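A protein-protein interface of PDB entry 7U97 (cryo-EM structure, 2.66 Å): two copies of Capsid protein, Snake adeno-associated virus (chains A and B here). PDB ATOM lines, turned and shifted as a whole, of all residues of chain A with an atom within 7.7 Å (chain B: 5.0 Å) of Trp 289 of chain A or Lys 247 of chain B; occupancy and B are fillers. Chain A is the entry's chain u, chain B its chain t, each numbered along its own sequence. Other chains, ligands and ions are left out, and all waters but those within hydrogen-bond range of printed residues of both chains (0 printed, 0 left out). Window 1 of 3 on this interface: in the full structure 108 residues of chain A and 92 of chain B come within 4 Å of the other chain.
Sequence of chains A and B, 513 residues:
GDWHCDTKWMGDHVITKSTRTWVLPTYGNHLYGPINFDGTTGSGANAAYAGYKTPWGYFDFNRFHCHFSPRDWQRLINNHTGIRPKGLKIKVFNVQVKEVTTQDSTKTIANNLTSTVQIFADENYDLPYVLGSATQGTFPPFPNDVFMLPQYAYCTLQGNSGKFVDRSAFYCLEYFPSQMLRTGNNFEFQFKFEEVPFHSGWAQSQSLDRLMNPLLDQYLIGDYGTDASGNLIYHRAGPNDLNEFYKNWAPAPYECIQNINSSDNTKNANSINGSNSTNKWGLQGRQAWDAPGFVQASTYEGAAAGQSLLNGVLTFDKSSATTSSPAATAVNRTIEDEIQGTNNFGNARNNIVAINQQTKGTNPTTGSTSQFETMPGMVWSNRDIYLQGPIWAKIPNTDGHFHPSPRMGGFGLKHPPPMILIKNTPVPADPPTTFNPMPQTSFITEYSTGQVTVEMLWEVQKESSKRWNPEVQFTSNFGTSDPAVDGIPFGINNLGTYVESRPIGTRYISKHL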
ATOM      1  N   ASN A  46     -12.910 -17.559 -21.446  1.00  0.00           N
ATOM      2  CA  ASN A  46     -11.819 -18.478 -21.721  1.00  0.00           C
ATOM      3  C   ASN A  46     -12.215 -19.596 -22.667  1.00  0.00           C
ATOM      4  O   ASN A  46     -11.339 -20.328 -23.129  1.00  0.00           O
ATOM      5  CB  ASN A  46     -11.294 -19.076 -20.418  1.00  0.00           C
ATOM      6  CG  ASN A  46     -10.554 -18.071 -19.572  1.00  0.00           C
ATOM      7  OD1 ASN A  46     -10.052 -17.073 -20.071  1.00  0.00           O
ATOM      8  ND2 ASN A  46     -10.479 -18.334 -18.280  1.00  0.00           N
ATOM      9  N   GLY A 132      -3.550 -34.878 -32.811  1.00  0.00           N
ATOM     10  CA  GLY A 132      -2.897 -35.093 -31.539  1.00  0.00           C
ATOM     11  C   GLY A 132      -3.608 -34.559 -30.315  1.00  0.00           C
ATOM     12  O   GLY A 132      -2.971 -34.422 -29.266  1.00  0.00           O
ATOM     13  N   SER A 133      -4.894 -34.251 -30.404  1.00  0.00           N
ATOM     14  CA  SER A 133      -5.616 -33.613 -29.314  1.00  0.00           C
ATOM     15  C   SER A 133      -6.400 -34.580 -28.444  1.00  0.00           C
ATOM     16  O   SER A 133      -7.124 -34.132 -27.553  1.00  0.00           O
ATOM     17  CB  SER A 133      -6.551 -32.548 -29.868  1.00  0.00           C
ATOM     18  OG  SER A 133      -5.796 -31.522 -30.484  1.00  0.00           O
ATOM     19  N   ALA A 134      -6.294 -35.883 -28.693  1.00  0.00           N
ATOM     20  CA  ALA A 134      -6.894 -36.910 -27.842  1.00  0.00           C
ATOM     21  C   ALA A 134      -8.409 -36.784 -27.772  1.00  0.00           C
ATOM     22  O   ALA A 134      -9.012 -36.945 -26.714  1.00  0.00           O
ATOM     23  CB  ALA A 134      -6.294 -36.892 -26.438  1.00  0.00           C
ATOM     24  N   ASN A 273     -13.701 -26.960  -5.991  1.00  0.00           N
ATOM     25  CA  ASN A 273     -14.036 -26.665  -7.377  1.00  0.00           C
ATOM     26  C   ASN A 273     -12.799 -26.947  -8.215  1.00  0.00           C
ATOM     27  O   ASN A 273     -11.817 -26.207  -8.147  1.00  0.00           O
ATOM     28  CB  ASN A 273     -14.494 -25.218  -7.522  1.00  0.00           C
ATOM     29  CG  ASN A 273     -15.042 -24.910  -8.894  1.00  0.00           C
ATOM     30  OD1 ASN A 273     -14.770 -25.616  -9.858  1.00  0.00           O
ATOM     31  ND2 ASN A 273     -15.824 -23.847  -8.987  1.00  0.00           N
ATOM     32  N   GLY A 274     -12.851 -28.014  -9.007  1.00  0.00           N
ATOM     33  CA  GLY A 274     -11.701 -28.418  -9.787  1.00  0.00           C
ATOM     34  C   GLY A 274     -11.284 -27.430 -10.844  1.00  0.00           C
ATOM     35  O   GLY A 274     -10.162 -27.524 -11.347  1.00  0.00           O
ATOM     36  N   SER A 275     -12.160 -26.498 -11.203  1.00  0.00           N
ATOM     37  CA  SER A 275     -11.788 -25.464 -12.153  1.00  0.00           C
ATOM     38  C   SER A 275     -10.945 -24.384 -11.500  1.00  0.00           C
ATOM     39  O   SER A 275     -10.070 -23.809 -12.153  1.00  0.00           O
ATOM     40  CB  SER A 275     -13.036 -24.844 -12.767  1.00  0.00           C
ATOM     41  OG  SER A 275     -13.766 -25.812 -13.493  1.00  0.00           O
ATOM     42  N   ASN A 276     -11.195 -24.089 -10.229  1.00  0.00           N
ATOM     43  CA  ASN A 276     -10.421 -23.066  -9.547  1.00  0.00           C
ATOM     44  C   ASN A 276      -9.073 -23.585  -9.076  1.00  0.00           C
ATOM     45  O   ASN A 276      -8.101 -22.825  -9.048  1.00  0.00           O
ATOM     46  CB  ASN A 276     -11.205 -22.519  -8.361  1.00  0.00           C
ATOM     47  CG  ASN A 276     -12.495 -21.869  -8.777  1.00  0.00           C
ATOM     48  OD1 ASN A 276     -13.540 -22.107  -8.182  1.00  0.00           O
ATOM     49  ND2 ASN A 276     -12.435 -21.058  -9.821  1.00  0.00           N
ATOM     50  N   SER A 277      -8.993 -24.854  -8.697  1.00  0.00           N
ATOM     51  CA  SER A 277      -7.792 -25.410  -8.095  1.00  0.00           C
ATOM     52  C   SER A 277      -6.882 -26.112  -9.091  1.00  0.00           C
ATOM     53  O   SER A 277      -5.879 -26.695  -8.682  1.00  0.00           O
ATOM     54  CB  SER A 277      -8.168 -26.371  -6.973  1.00  0.00           C
ATOM     55  OG  SER A 277      -8.900 -27.465  -7.482  1.00  0.00           O
ATOM     56  N   THR A 278      -7.204 -26.085 -10.374  1.00  0.00           N
ATOM     57  CA  THR A 278      -6.321 -26.646 -11.383  1.00  0.00           C
ATOM     58  C   THR A 278      -5.232 -25.644 -11.747  1.00  0.00           C
ATOM     59  O   THR A 278      -5.427 -24.431 -11.669  1.00  0.00           O
ATOM     60  CB  THR A 278      -7.125 -27.037 -12.623  1.00  0.00           C
ATOM     61  OG1 THR A 278      -8.166 -27.937 -12.245  1.00  0.00           O
ATOM     62  CG2 THR A 278      -6.257 -27.738 -13.635  1.00  0.00           C
ATOM     63  N   ASN A 279      -4.066 -26.160 -12.122  1.00  0.00           N
ATOM     64  CA  ASN A 279      -3.036 -25.313 -12.701  1.00  0.00           C
ATOM     65  C   ASN A 279      -3.489 -24.786 -14.050  1.00  0.00           C
ATOM     66  O   ASN A 279      -4.064 -25.515 -14.859  1.00  0.00           O
ATOM     67  CB  ASN A 279      -1.730 -26.077 -12.880  1.00  0.00           C
ATOM     68  CG  ASN A 279      -1.090 -26.446 -11.577  1.00  0.00           C
ATOM     69  OD1 ASN A 279      -1.430 -25.908 -10.534  1.00  0.00           O
ATOM     70  ND2 ASN A 279      -0.120 -27.337 -11.634  1.00  0.00           N
ATOM     71  N   LYS A 280      -3.207 -23.516 -14.301  1.00  0.00           N
ATOM     72  CA  LYS A 280      -3.524 -22.871 -15.559  1.00  0.00           C
ATOM     73  C   LYS A 280      -2.234 -22.409 -16.214  1.00  0.00           C
ATOM     74  O   LYS A 280      -1.234 -22.170 -15.540  1.00  0.00           O
ATOM     75  CB  LYS A 280      -4.405 -21.649 -15.350  1.00  0.00           C
ATOM     76  CG  LYS A 280      -5.631 -21.876 -14.517  1.00  0.00           C
ATOM     77  CD  LYS A 280      -6.656 -22.719 -15.190  1.00  0.00           C
ATOM     78  CE  LYS A 280      -7.818 -22.887 -14.255  1.00  0.00           C
ATOM     79  NZ  LYS A 280      -8.401 -21.566 -13.937  1.00  0.00           N
ATOM     80  N   TRP A 281      -2.258 -22.281 -17.531  1.00  0.00           N
ATOM     81  CA  TRP A 281      -1.338 -21.396 -18.223  1.00  0.00           C
ATOM     82  C   TRP A 281      -2.145 -20.465 -19.102  1.00  0.00           C
ATOM     83  O   TRP A 281      -3.055 -20.905 -19.802  1.00  0.00           O
ATOM     84  CB  TRP A 281      -0.283 -22.129 -19.052  1.00  0.00           C
ATOM     85  CG  TRP A 281      -0.726 -23.145 -20.046  1.00  0.00           C
ATOM     86  CD1 TRP A 281      -0.713 -24.489 -19.882  1.00  0.00           C
ATOM     87  CD2 TRP A 281      -1.225 -22.907 -21.363  1.00  0.00           C
ATOM     88  NE1 TRP A 281      -1.159 -25.111 -21.013  1.00  0.00           N
ATOM     89  CE2 TRP A 281      -1.486 -24.158 -21.938  1.00  0.00           C
ATOM     90  CE3 TRP A 281      -1.476 -21.758 -22.115  1.00  0.00           C
ATOM     91  CZ2 TRP A 281      -1.987 -24.294 -23.222  1.00  0.00           C
ATOM     92  CZ3 TRP A 281      -1.968 -21.896 -23.383  1.00  0.00           C
ATOM     93  CH2 TRP A 281      -2.220 -23.152 -23.926  1.00  0.00           C
ATOM     94  N   GLY A 282      -1.844 -19.183 -19.024  1.00  0.00           N
ATOM     95  CA  GLY A 282      -2.524 -18.211 -19.835  1.00  0.00           C
ATOM     96  C   GLY A 282      -1.816 -17.955 -21.144  1.00  0.00           C
ATOM     97  O   GLY A 282      -0.605 -18.077 -21.253  1.00  0.00           O
ATOM     98  N   GLN A 287      -6.842 -17.920 -20.315  1.00  0.00           N
ATOM     99  CA  GLN A 287      -6.026 -18.945 -19.679  1.00  0.00           C
ATOM    100  C   GLN A 287      -6.699 -20.307 -19.717  1.00  0.00           C
ATOM    101  O   GLN A 287      -7.892 -20.435 -19.434  1.00  0.00           O
ATOM    102  CB  GLN A 287      -5.689 -18.545 -18.255  1.00  0.00           C
ATOM    103  CG  GLN A 287      -6.870 -18.241 -17.398  1.00  0.00           C
ATOM    104  CD  GLN A 287      -6.460 -17.766 -16.036  1.00  0.00           C
ATOM    105  OE1 GLN A 287      -5.316 -17.381 -15.828  1.00  0.00           O
ATOM    106  NE2 GLN A 287      -7.395 -17.770 -15.097  1.00  0.00           N
ATOM    107  N   ALA A 288      -5.911 -21.325 -20.059  1.00  0.00           N
ATOM    108  CA  ALA A 288      -6.381 -22.684 -20.273  1.00  0.00           C
ATOM    109  C   ALA A 288      -5.782 -23.619 -19.236  1.00  0.00           C
ATOM    110  O   ALA A 288      -4.711 -23.355 -18.692  1.00  0.00           O
ATOM    111  CB  ALA A 288      -6.007 -23.180 -21.669  1.00  0.00           C
ATOM    112  N   TRP A 289      -6.486 -24.714 -18.965  1.00  0.00           N
ATOM    113  CA  TRP A 289      -5.969 -25.723 -18.057  1.00  0.00           C
ATOM    114  C   TRP A 289      -4.597 -26.197 -18.498  1.00  0.00           C
ATOM    115  O   TRP A 289      -4.384 -26.528 -19.665  1.00  0.00           O
ATOM    116  CB  TRP A 289      -6.907 -26.924 -17.982  1.00  0.00           C
ATOM    117  CG  TRP A 289      -8.105 -26.711 -17.176  1.00  0.00           C
ATOM    118  CD1 TRP A 289      -8.568 -25.534 -16.688  1.00  0.00           C
ATOM    119  CD2 TRP A 289      -8.934 -27.730 -16.628  1.00  0.00           C
ATOM    120  NE1 TRP A 289      -9.685 -25.752 -15.929  1.00  0.00           N
ATOM    121  CE2 TRP A 289      -9.923 -27.098 -15.867  1.00  0.00           C
ATOM    122  CE3 TRP A 289      -8.949 -29.115 -16.733  1.00  0.00           C
ATOM    123  CZ2 TRP A 289     -10.904 -27.802 -15.203  1.00  0.00           C
ATOM    124  CZ3 TRP A 289      -9.930 -29.810 -16.087  1.00  0.00           C
ATOM    125  CH2 TRP A 289     -10.893 -29.159 -15.332  1.00  0.00           C
ATOM    126  N   ASP A 290      -3.669 -26.249 -17.553  1.00  0.00           N
ATOM    127  CA  ASP A 290      -2.405 -26.932 -17.787  1.00  0.00           C
ATOM    128  C   ASP A 290      -2.603 -28.345 -17.284  1.00  0.00           C
ATOM    129  O   ASP A 290      -2.557 -28.603 -16.082  1.00  0.00           O
ATOM    130  CB  ASP A 290      -1.268 -26.234 -17.055  1.00  0.00           C
ATOM    131  CG  ASP A 290       0.077 -26.858 -17.333  1.00  0.00           C
ATOM    132  OD1 ASP A 290       0.156 -27.799 -18.151  1.00  0.00           O
ATOM    133  OD2 ASP A 290       1.072 -26.407 -16.735  1.00  0.00           O
ATOM    134  N   ALA A 291      -2.806 -29.271 -18.202  1.00  0.00           N
ATOM    135  CA  ALA A 291      -3.053 -30.632 -17.796  1.00  0.00           C
ATOM    136  C   ALA A 291      -2.576 -31.587 -18.855  1.00  0.00           C
ATOM    137  O   ALA A 291      -2.724 -31.315 -20.035  1.00  0.00           O
ATOM    138  CB  ALA A 291      -4.507 -30.822 -17.514  1.00  0.00           C
ATOM    139  N   PRO A 292      -2.031 -32.731 -18.438  1.00  0.00           N
ATOM    140  CA  PRO A 292      -1.719 -33.100 -17.058  1.00  0.00           C
ATOM    141  C   PRO A 292      -0.556 -32.296 -16.483  1.00  0.00           C
ATOM    142  O   PRO A 292      -0.353 -32.267 -15.277  1.00  0.00           O
ATOM    143  CB  PRO A 292      -1.334 -34.568 -17.175  1.00  0.00           C
ATOM    144  CG  PRO A 292      -1.939 -35.014 -18.440  1.00  0.00           C
ATOM    145  CD  PRO A 292      -1.810 -33.857 -19.350  1.00  0.00           C
ATOM    146  N   GLY A 293       0.193 -31.649 -17.355  1.00  0.00           N
ATOM    147  CA  GLY A 293       1.403 -30.963 -16.969  1.00  0.00           C
ATOM    148  C   GLY A 293       2.611 -31.832 -17.227  1.00  0.00           C
ATOM    149  O   GLY A 293       2.542 -32.873 -17.882  1.00  0.00           O
ATOM    150  N   LEU A 310      -4.520 -33.885  -8.724  1.00  0.00           N
ATOM    151  CA  LEU A 310      -5.731 -33.359  -9.336  1.00  0.00           C
ATOM    152  C   LEU A 310      -5.408 -32.872 -10.739  1.00  0.00           C
ATOM    153  O   LEU A 310      -4.656 -31.910 -10.910  1.00  0.00           O
ATOM    154  CB  LEU A 310      -6.313 -32.239  -8.483  1.00  0.00           C
ATOM    155  CG  LEU A 310      -7.659 -31.672  -8.911  1.00  0.00           C
ATOM    156  CD1 LEU A 310      -8.473 -31.344  -7.702  1.00  0.00           C
ATOM    157  CD2 LEU A 310      -7.448 -30.423  -9.711  1.00  0.00           C
ATOM    158  N   ASN A 311      -6.003 -33.525 -11.736  1.00  0.00           N
ATOM    159  CA  ASN A 311      -5.690 -33.300 -13.143  1.00  0.00           C
ATOM    160  C   ASN A 311      -4.212 -33.510 -13.435  1.00  0.00           C
ATOM    161  O   ASN A 311      -3.650 -32.868 -14.321  1.00  0.00           O
ATOM    162  CB  ASN A 311      -6.132 -31.912 -13.598  1.00  0.00           C
ATOM    163  CG  ASN A 311      -7.624 -31.765 -13.606  1.00  0.00           C
ATOM    164  OD1 ASN A 311      -8.170 -30.815 -13.059  1.00  0.00           O
ATOM    165  ND2 ASN A 311      -8.298 -32.706 -14.239  1.00  0.00           N
ATOM    166  N   PRO A 406       5.618 -35.291 -25.750  1.00  0.00           N
ATOM    167  CA  PRO A 406       4.235 -34.915 -25.448  1.00  0.00           C
ATOM    168  C   PRO A 406       3.891 -35.143 -23.987  1.00  0.00           C
ATOM    169  O   PRO A 406       4.332 -36.108 -23.368  1.00  0.00           O
ATOM    170  CB  PRO A 406       3.422 -35.835 -26.359  1.00  0.00           C
ATOM    171  CG  PRO A 406       4.333 -36.174 -27.443  1.00  0.00           C
ATOM    172  CD  PRO A 406       5.679 -36.288 -26.827  1.00  0.00           C
ATOM    173  N   ARG A 407       3.089 -34.241 -23.440  1.00  0.00           N
ATOM    174  CA  ARG A 407       2.748 -34.319 -22.032  1.00  0.00           C
ATOM    175  C   ARG A 407       1.656 -35.329 -21.732  1.00  0.00           C
ATOM    176  O   ARG A 407       1.534 -35.755 -20.581  1.00  0.00           O
ATOM    177  CB  ARG A 407       2.334 -32.947 -21.513  1.00  0.00           C
ATOM    178  CG  ARG A 407       3.485 -31.996 -21.368  1.00  0.00           C
ATOM    179  CD  ARG A 407       3.027 -30.741 -20.701  1.00  0.00           C
ATOM    180  NE  ARG A 407       4.137 -29.874 -20.356  1.00  0.00           N
ATOM    181  CZ  ARG A 407       3.998 -28.710 -19.743  1.00  0.00           C
ATOM    182  NH1 ARG A 407       2.794 -28.280 -19.411  1.00  0.00           N
ATOM    183  NH2 ARG A 407       5.062 -27.986 -19.452  1.00  0.00           N
ATOM    184  N   MET A 408       0.856 -35.714 -22.720  1.00  0.00           N
ATOM    185  CA  MET A 408      -0.080 -36.808 -22.504  1.00  0.00           C
ATOM    186  C   MET A 408       0.633 -38.147 -22.558  1.00  0.00           C
ATOM    187  O   MET A 408       0.335 -39.049 -21.774  1.00  0.00           O
ATOM    188  CB  MET A 408      -1.186 -36.779 -23.548  1.00  0.00           C
ATOM    189  CG  MET A 408      -2.080 -35.564 -23.543  1.00  0.00           C
ATOM    190  SD  MET A 408      -3.199 -35.748 -24.936  1.00  0.00           S
ATOM    191  CE  MET A 408      -4.071 -34.202 -24.926  1.00  0.00           C
ATOM    192  N   GLY A 409       1.533 -38.301 -23.503  1.00  0.00           N
ATOM    193  CA  GLY A 409       2.368 -39.478 -23.603  1.00  0.00           C
ATOM    194  C   GLY A 409       2.691 -39.729 -25.057  1.00  0.00           C
ATOM    195  O   GLY A 409       2.169 -39.080 -25.953  1.00  0.00           O
ATOM    196  N   LEU B 208      -1.853 -22.218 -29.229  1.00  0.00           N
ATOM    197  CA  LEU B 208      -1.614 -23.493 -28.565  1.00  0.00           C
ATOM    198  C   LEU B 208      -2.857 -23.991 -27.856  1.00  0.00           C
ATOM    199  O   LEU B 208      -3.134 -25.194 -27.857  1.00  0.00           O
ATOM    200  CB  LEU B 208      -0.467 -23.385 -27.570  1.00  0.00           C
ATOM    201  CG  LEU B 208       0.934 -23.319 -28.147  1.00  0.00           C
ATOM    202  CD1 LEU B 208       1.898 -23.137 -27.027  1.00  0.00           C
ATOM    203  CD2 LEU B 208       1.227 -24.600 -28.886  1.00  0.00           C
ATOM    204  N   ASP B 209      -3.613 -23.093 -27.238  1.00  0.00           N
ATOM    205  CA  ASP B 209      -4.763 -23.549 -26.480  1.00  0.00           C
ATOM    206  C   ASP B 209      -5.886 -24.046 -27.370  1.00  0.00           C
ATOM    207  O   ASP B 209      -6.762 -24.756 -26.876  1.00  0.00           O
ATOM    208  CB  ASP B 209      -5.259 -22.453 -25.543  1.00  0.00           C
ATOM    209  CG  ASP B 209      -5.609 -21.183 -26.262  1.00  0.00           C
ATOM    210  OD1 ASP B 209      -5.345 -21.088 -27.472  1.00  0.00           O
ATOM    211  OD2 ASP B 209      -6.150 -20.270 -25.612  1.00  0.00           O
ATOM    212  N   ASP B 223     -10.976 -33.966 -13.804  1.00  0.00           N
ATOM    213  CA  ASP B 223     -11.360 -33.921 -12.399  1.00  0.00           C
ATOM    214  C   ASP B 223     -12.129 -32.632 -12.175  1.00  0.00           C
ATOM    215  O   ASP B 223     -11.546 -31.545 -12.196  1.00  0.00           O
ATOM    216  CB  ASP B 223     -10.137 -33.992 -11.490  1.00  0.00           C
ATOM    217  CG  ASP B 223      -9.416 -35.309 -11.594  1.00  0.00           C
ATOM    218  OD1 ASP B 223      -9.997 -36.261 -12.147  1.00  0.00           O
ATOM    219  OD2 ASP B 223      -8.266 -35.395 -11.127  1.00  0.00           O
ATOM    220  N   LEU B 242     -13.544 -25.529 -24.094  1.00  0.00           N
ATOM    221  CA  LEU B 242     -12.332 -26.037 -24.714  1.00  0.00           C
ATOM    222  C   LEU B 242     -11.089 -25.752 -23.900  1.00  0.00           C
ATOM    223  O   LEU B 242     -10.032 -26.302 -24.212  1.00  0.00           O
ATOM    224  CB  LEU B 242     -12.148 -25.449 -26.109  1.00  0.00           C
ATOM    225  CG  LEU B 242     -13.160 -25.792 -27.191  1.00  0.00           C
ATOM    226  CD1 LEU B 242     -12.820 -25.000 -28.411  1.00  0.00           C
ATOM    227  CD2 LEU B 242     -13.167 -27.252 -27.523  1.00  0.00           C
ATOM    228  N   ASN B 243     -11.178 -24.907 -22.879  1.00  0.00           N
ATOM    229  CA  ASN B 243     -10.053 -24.703 -21.981  1.00  0.00           C
ATOM    230  C   ASN B 243      -9.802 -25.899 -21.076  1.00  0.00           C
ATOM    231  O   ASN B 243      -8.724 -25.999 -20.487  1.00  0.00           O
ATOM    232  CB  ASN B 243     -10.291 -23.448 -21.149  1.00  0.00           C
ATOM    233  CG  ASN B 243     -11.601 -23.482 -20.422  1.00  0.00           C
ATOM    234  OD1 ASN B 243     -12.114 -24.535 -20.098  1.00  0.00           O
ATOM    235  ND2 ASN B 243     -12.141 -22.319 -20.139  1.00  0.00           N
ATOM    236  N   GLU B 244     -10.777 -26.793 -20.958  1.00  0.00           N
ATOM    237  CA  GLU B 244     -10.723 -27.970 -20.108  1.00  0.00           C
ATOM    238  C   GLU B 244      -9.891 -29.083 -20.712  1.00  0.00           C
ATOM    239  O   GLU B 244      -9.485 -29.994 -19.989  1.00  0.00           O
ATOM    240  CB  GLU B 244     -12.142 -28.479 -19.919  1.00  0.00           C
ATOM    241  CG  GLU B 244     -13.071 -27.404 -19.471  1.00  0.00           C
ATOM    242  CD  GLU B 244     -12.899 -27.007 -18.054  1.00  0.00           C
ATOM    243  OE1 GLU B 244     -12.843 -27.920 -17.240  1.00  0.00           O
ATOM    244  OE2 GLU B 244     -12.833 -25.808 -17.770  1.00  0.00           O
ATOM    245  N   PHE B 245      -9.710 -29.061 -22.030  1.00  0.00           N
ATOM    246  CA  PHE B 245      -8.957 -30.079 -22.747  1.00  0.00           C
ATOM    247  C   PHE B 245      -7.596 -30.310 -22.123  1.00  0.00           C
ATOM    248  O   PHE B 245      -6.913 -29.366 -21.733  1.00  0.00           O
ATOM    249  CB  PHE B 245      -8.791 -29.645 -24.205  1.00  0.00           C
ATOM    250  CG  PHE B 245      -9.922 -30.048 -25.091  1.00  0.00           C
ATOM    251  CD1 PHE B 245      -9.758 -31.061 -26.005  1.00  0.00           C
ATOM    252  CD2 PHE B 245     -11.174 -29.518 -24.931  1.00  0.00           C
ATOM    253  CE1 PHE B 245     -10.799 -31.468 -26.810  1.00  0.00           C
ATOM    254  CE2 PHE B 245     -12.221 -29.940 -25.726  1.00  0.00           C
ATOM    255  CZ  PHE B 245     -12.032 -30.913 -26.666  1.00  0.00           C
ATOM    256  N   TYR B 246      -7.207 -31.575 -22.022  1.00  0.00           N
ATOM    257  CA  TYR B 246      -5.805 -31.873 -21.806  1.00  0.00           C
ATOM    258  C   TYR B 246      -5.030 -31.551 -23.071  1.00  0.00           C
ATOM    259  O   TYR B 246      -5.585 -31.529 -24.169  1.00  0.00           O
ATOM    260  CB  TYR B 246      -5.581 -33.333 -21.412  1.00  0.00           C
ATOM    261  CG  TYR B 246      -6.154 -33.712 -20.075  1.00  0.00           C
ATOM    262  CD1 TYR B 246      -6.622 -32.753 -19.211  1.00  0.00           C
ATOM    263  CD2 TYR B 246      -6.044 -34.995 -19.602  1.00  0.00           C
ATOM    264  CE1 TYR B 246      -7.100 -33.080 -17.969  1.00  0.00           C
ATOM    265  CE2 TYR B 246      -6.495 -35.324 -18.354  1.00  0.00           C
ATOM    266  CZ  TYR B 246      -7.020 -34.358 -17.538  1.00  0.00           C
ATOM    267  OH  TYR B 246      -7.482 -34.675 -16.287  1.00  0.00           O
ATOM    268  N   LYS B 247      -3.742 -31.288 -22.915  1.00  0.00           N
ATOM    269  CA  LYS B 247      -2.933 -30.805 -24.019  1.00  0.00           C
ATOM    270  C   LYS B 247      -1.521 -31.347 -23.891  1.00  0.00           C
ATOM    271  O   LYS B 247      -1.033 -31.585 -22.788  1.00  0.00           O
ATOM    272  CB  LYS B 247      -2.949 -29.276 -24.063  1.00  0.00           C
ATOM    273  CG  LYS B 247      -4.254 -28.721 -24.591  1.00  0.00           C
ATOM    274  CD  LYS B 247      -4.340 -27.237 -24.482  1.00  0.00           C
ATOM    275  CE  LYS B 247      -4.537 -26.835 -23.056  1.00  0.00           C
ATOM    276  NZ  LYS B 247      -5.841 -27.310 -22.567  1.00  0.00           N
ATOM    277  N   ASN B 248      -0.880 -31.576 -25.036  1.00  0.00           N
ATOM    278  CA  ASN B 248       0.470 -32.113 -25.053  1.00  0.00           C
ATOM    279  C   ASN B 248       1.541 -31.058 -24.840  1.00  0.00           C
ATOM    280  O   ASN B 248       2.669 -31.413 -24.496  1.00  0.00           O
ATOM    281  CB  ASN B 248       0.764 -32.813 -26.379  1.00  0.00           C
ATOM    282  CG  ASN B 248       0.015 -34.104 -26.540  1.00  0.00           C
ATOM    283  OD1 ASN B 248       0.346 -35.109 -25.923  1.00  0.00           O
ATOM    284  ND2 ASN B 248      -0.977 -34.100 -27.411  1.00  0.00           N
ATOM    285  N   TRP B 249       1.242 -29.784 -25.060  1.00  0.00           N
ATOM    286  CA  TRP B 249       2.280 -28.772 -25.107  1.00  0.00           C
ATOM    287  C   TRP B 249       1.878 -27.597 -24.232  1.00  0.00           C
ATOM    288  O   TRP B 249       0.724 -27.472 -23.827  1.00  0.00           O
ATOM    289  CB  TRP B 249       2.527 -28.311 -26.548  1.00  0.00           C
ATOM    290  CG  TRP B 249       2.757 -29.459 -27.469  1.00  0.00           C
ATOM    291  CD1 TRP B 249       1.899 -29.936 -28.406  1.00  0.00           C
ATOM    292  CD2 TRP B 249       3.874 -30.346 -27.467  1.00  0.00           C
ATOM    293  NE1 TRP B 249       2.435 -31.031 -29.027  1.00  0.00           N
ATOM    294  CE2 TRP B 249       3.647 -31.307 -28.461  1.00  0.00           C
ATOM    295  CE3 TRP B 249       5.058 -30.407 -26.732  1.00  0.00           C
ATOM    296  CZ2 TRP B 249       4.555 -32.309 -28.739  1.00  0.00           C
ATOM    297  CZ3 TRP B 249       5.948 -31.397 -27.008  1.00  0.00           C
ATOM    298  CH2 TRP B 249       5.699 -32.335 -28.002  1.00  0.00           C
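The backbone carbonyl oxygen of Ala 291 of chain A lies within hydrogen-bond range of the backbone NH of Lys 247 of chain B, at 3.1 Å. The backbone carbonyl oxygen of Asn 248 of chain B sits at hydrogen-bond distance from the backbone NH of Arg 407 of chain A (3.0 Å). The side-chain amide nitrogen of Asn 248 of chain B lies within hydrogen-bond range of the backbone carbonyl oxygen of Gly 132 of chain A (2.7 Å). OH of Tyr 246 of chain B sits at hydrogen-bond distance from ND2 of Asn 311 of chain A, at 3.0 Å. N of Met 408 of chain A lies close to OD1 of Asn 248 of chain B (3.3 Å). The side-chain amino group (NZ) of Lys 247 of chain B sits at hydrogen-bond distance from the backbone carbonyl oxygen (O) of Trp 289 of chain A. O of Asn 243 of chain B sits at hydrogen-bond distance from N of Trp 289 of chain A, 3.0 Å away. N of Asp 223 of chain B lies close to ND2 of Asn 311 of chain A.
The backbone carbonyl oxygen of Phe 245 of chain B is in hydrogen-bond range of the side-chain amino group of Lys 247 of chain B (2.5 Å). The side-chain amide oxygen (OD1) of Asn 46 of chain A lies within hydrogen-bond range of the backbone NH (N) of Gln 287 of chain A (3.3 Å).
Among the printed residues, merely in contact across the chains: Asn 46 of chain A with Asn 243 of chain B, Gly 274 of chain A with Asp 223 of chain B, Trp 281 of chain A with Asp 209 of chain B, Trp 281 of chain A with Lys 247 of chain B, Ala 288 of chain A with Asn 243 of chain B, Trp 289 of chain A with Asp 223 of chain B, Trp 289 of chain A with Glu 244 of chain B, Ala 291 of chain A with Tyr 246 of chain B, Leu 310 of chain A with Asp 223 of chain B, Pro 406 of chain A with Asn 248 of chain B, Pro 406 of chain A with Trp 249 of chain B, Arg 407 of chain A with Lys 247 of chain B, Met 408 of chain A with Tyr 246 of chain B and Met 408 of chain A with Lys 247 of chain B.
Of the printed residues of chain B, Trp 289 of chain A touches Asp 223 (3.99 Å), Asn 243 (3.0 Å), Glu 244 (2.8 Å) and Lys 247 (3.3 Å). Lys 247 of chain B touches five residues of chain A. Printed residues of chain B within 4 Å of Asn 46 of chain A: Asn 243 (3.4 Å). Printed residues of chain A within 4 Å of Asn 243 of chain B: Asn 46, Ala 288 and Trp 289. Of the printed residues of chain B, Leu 310 of chain A touches Asp 223. The nearest printed residue of chain B that does not touch Trp 289 of chain A is Phe 245 of chain B (4.3 Å). The nearest printed residue of chain A that does not touch Lys 247 of chain B is Ala 288 of chain A (4.2 Å).
Hydrophobic or aromatic side chains of chain A within 4 Å of the printed part of chain B: Trp 281, Trp 289, Ala 291, Pro 406 and Met 408. Of the 11 printed residues of chain B, 8 touch a printed residue of chain A.
No position is printed for both chains.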
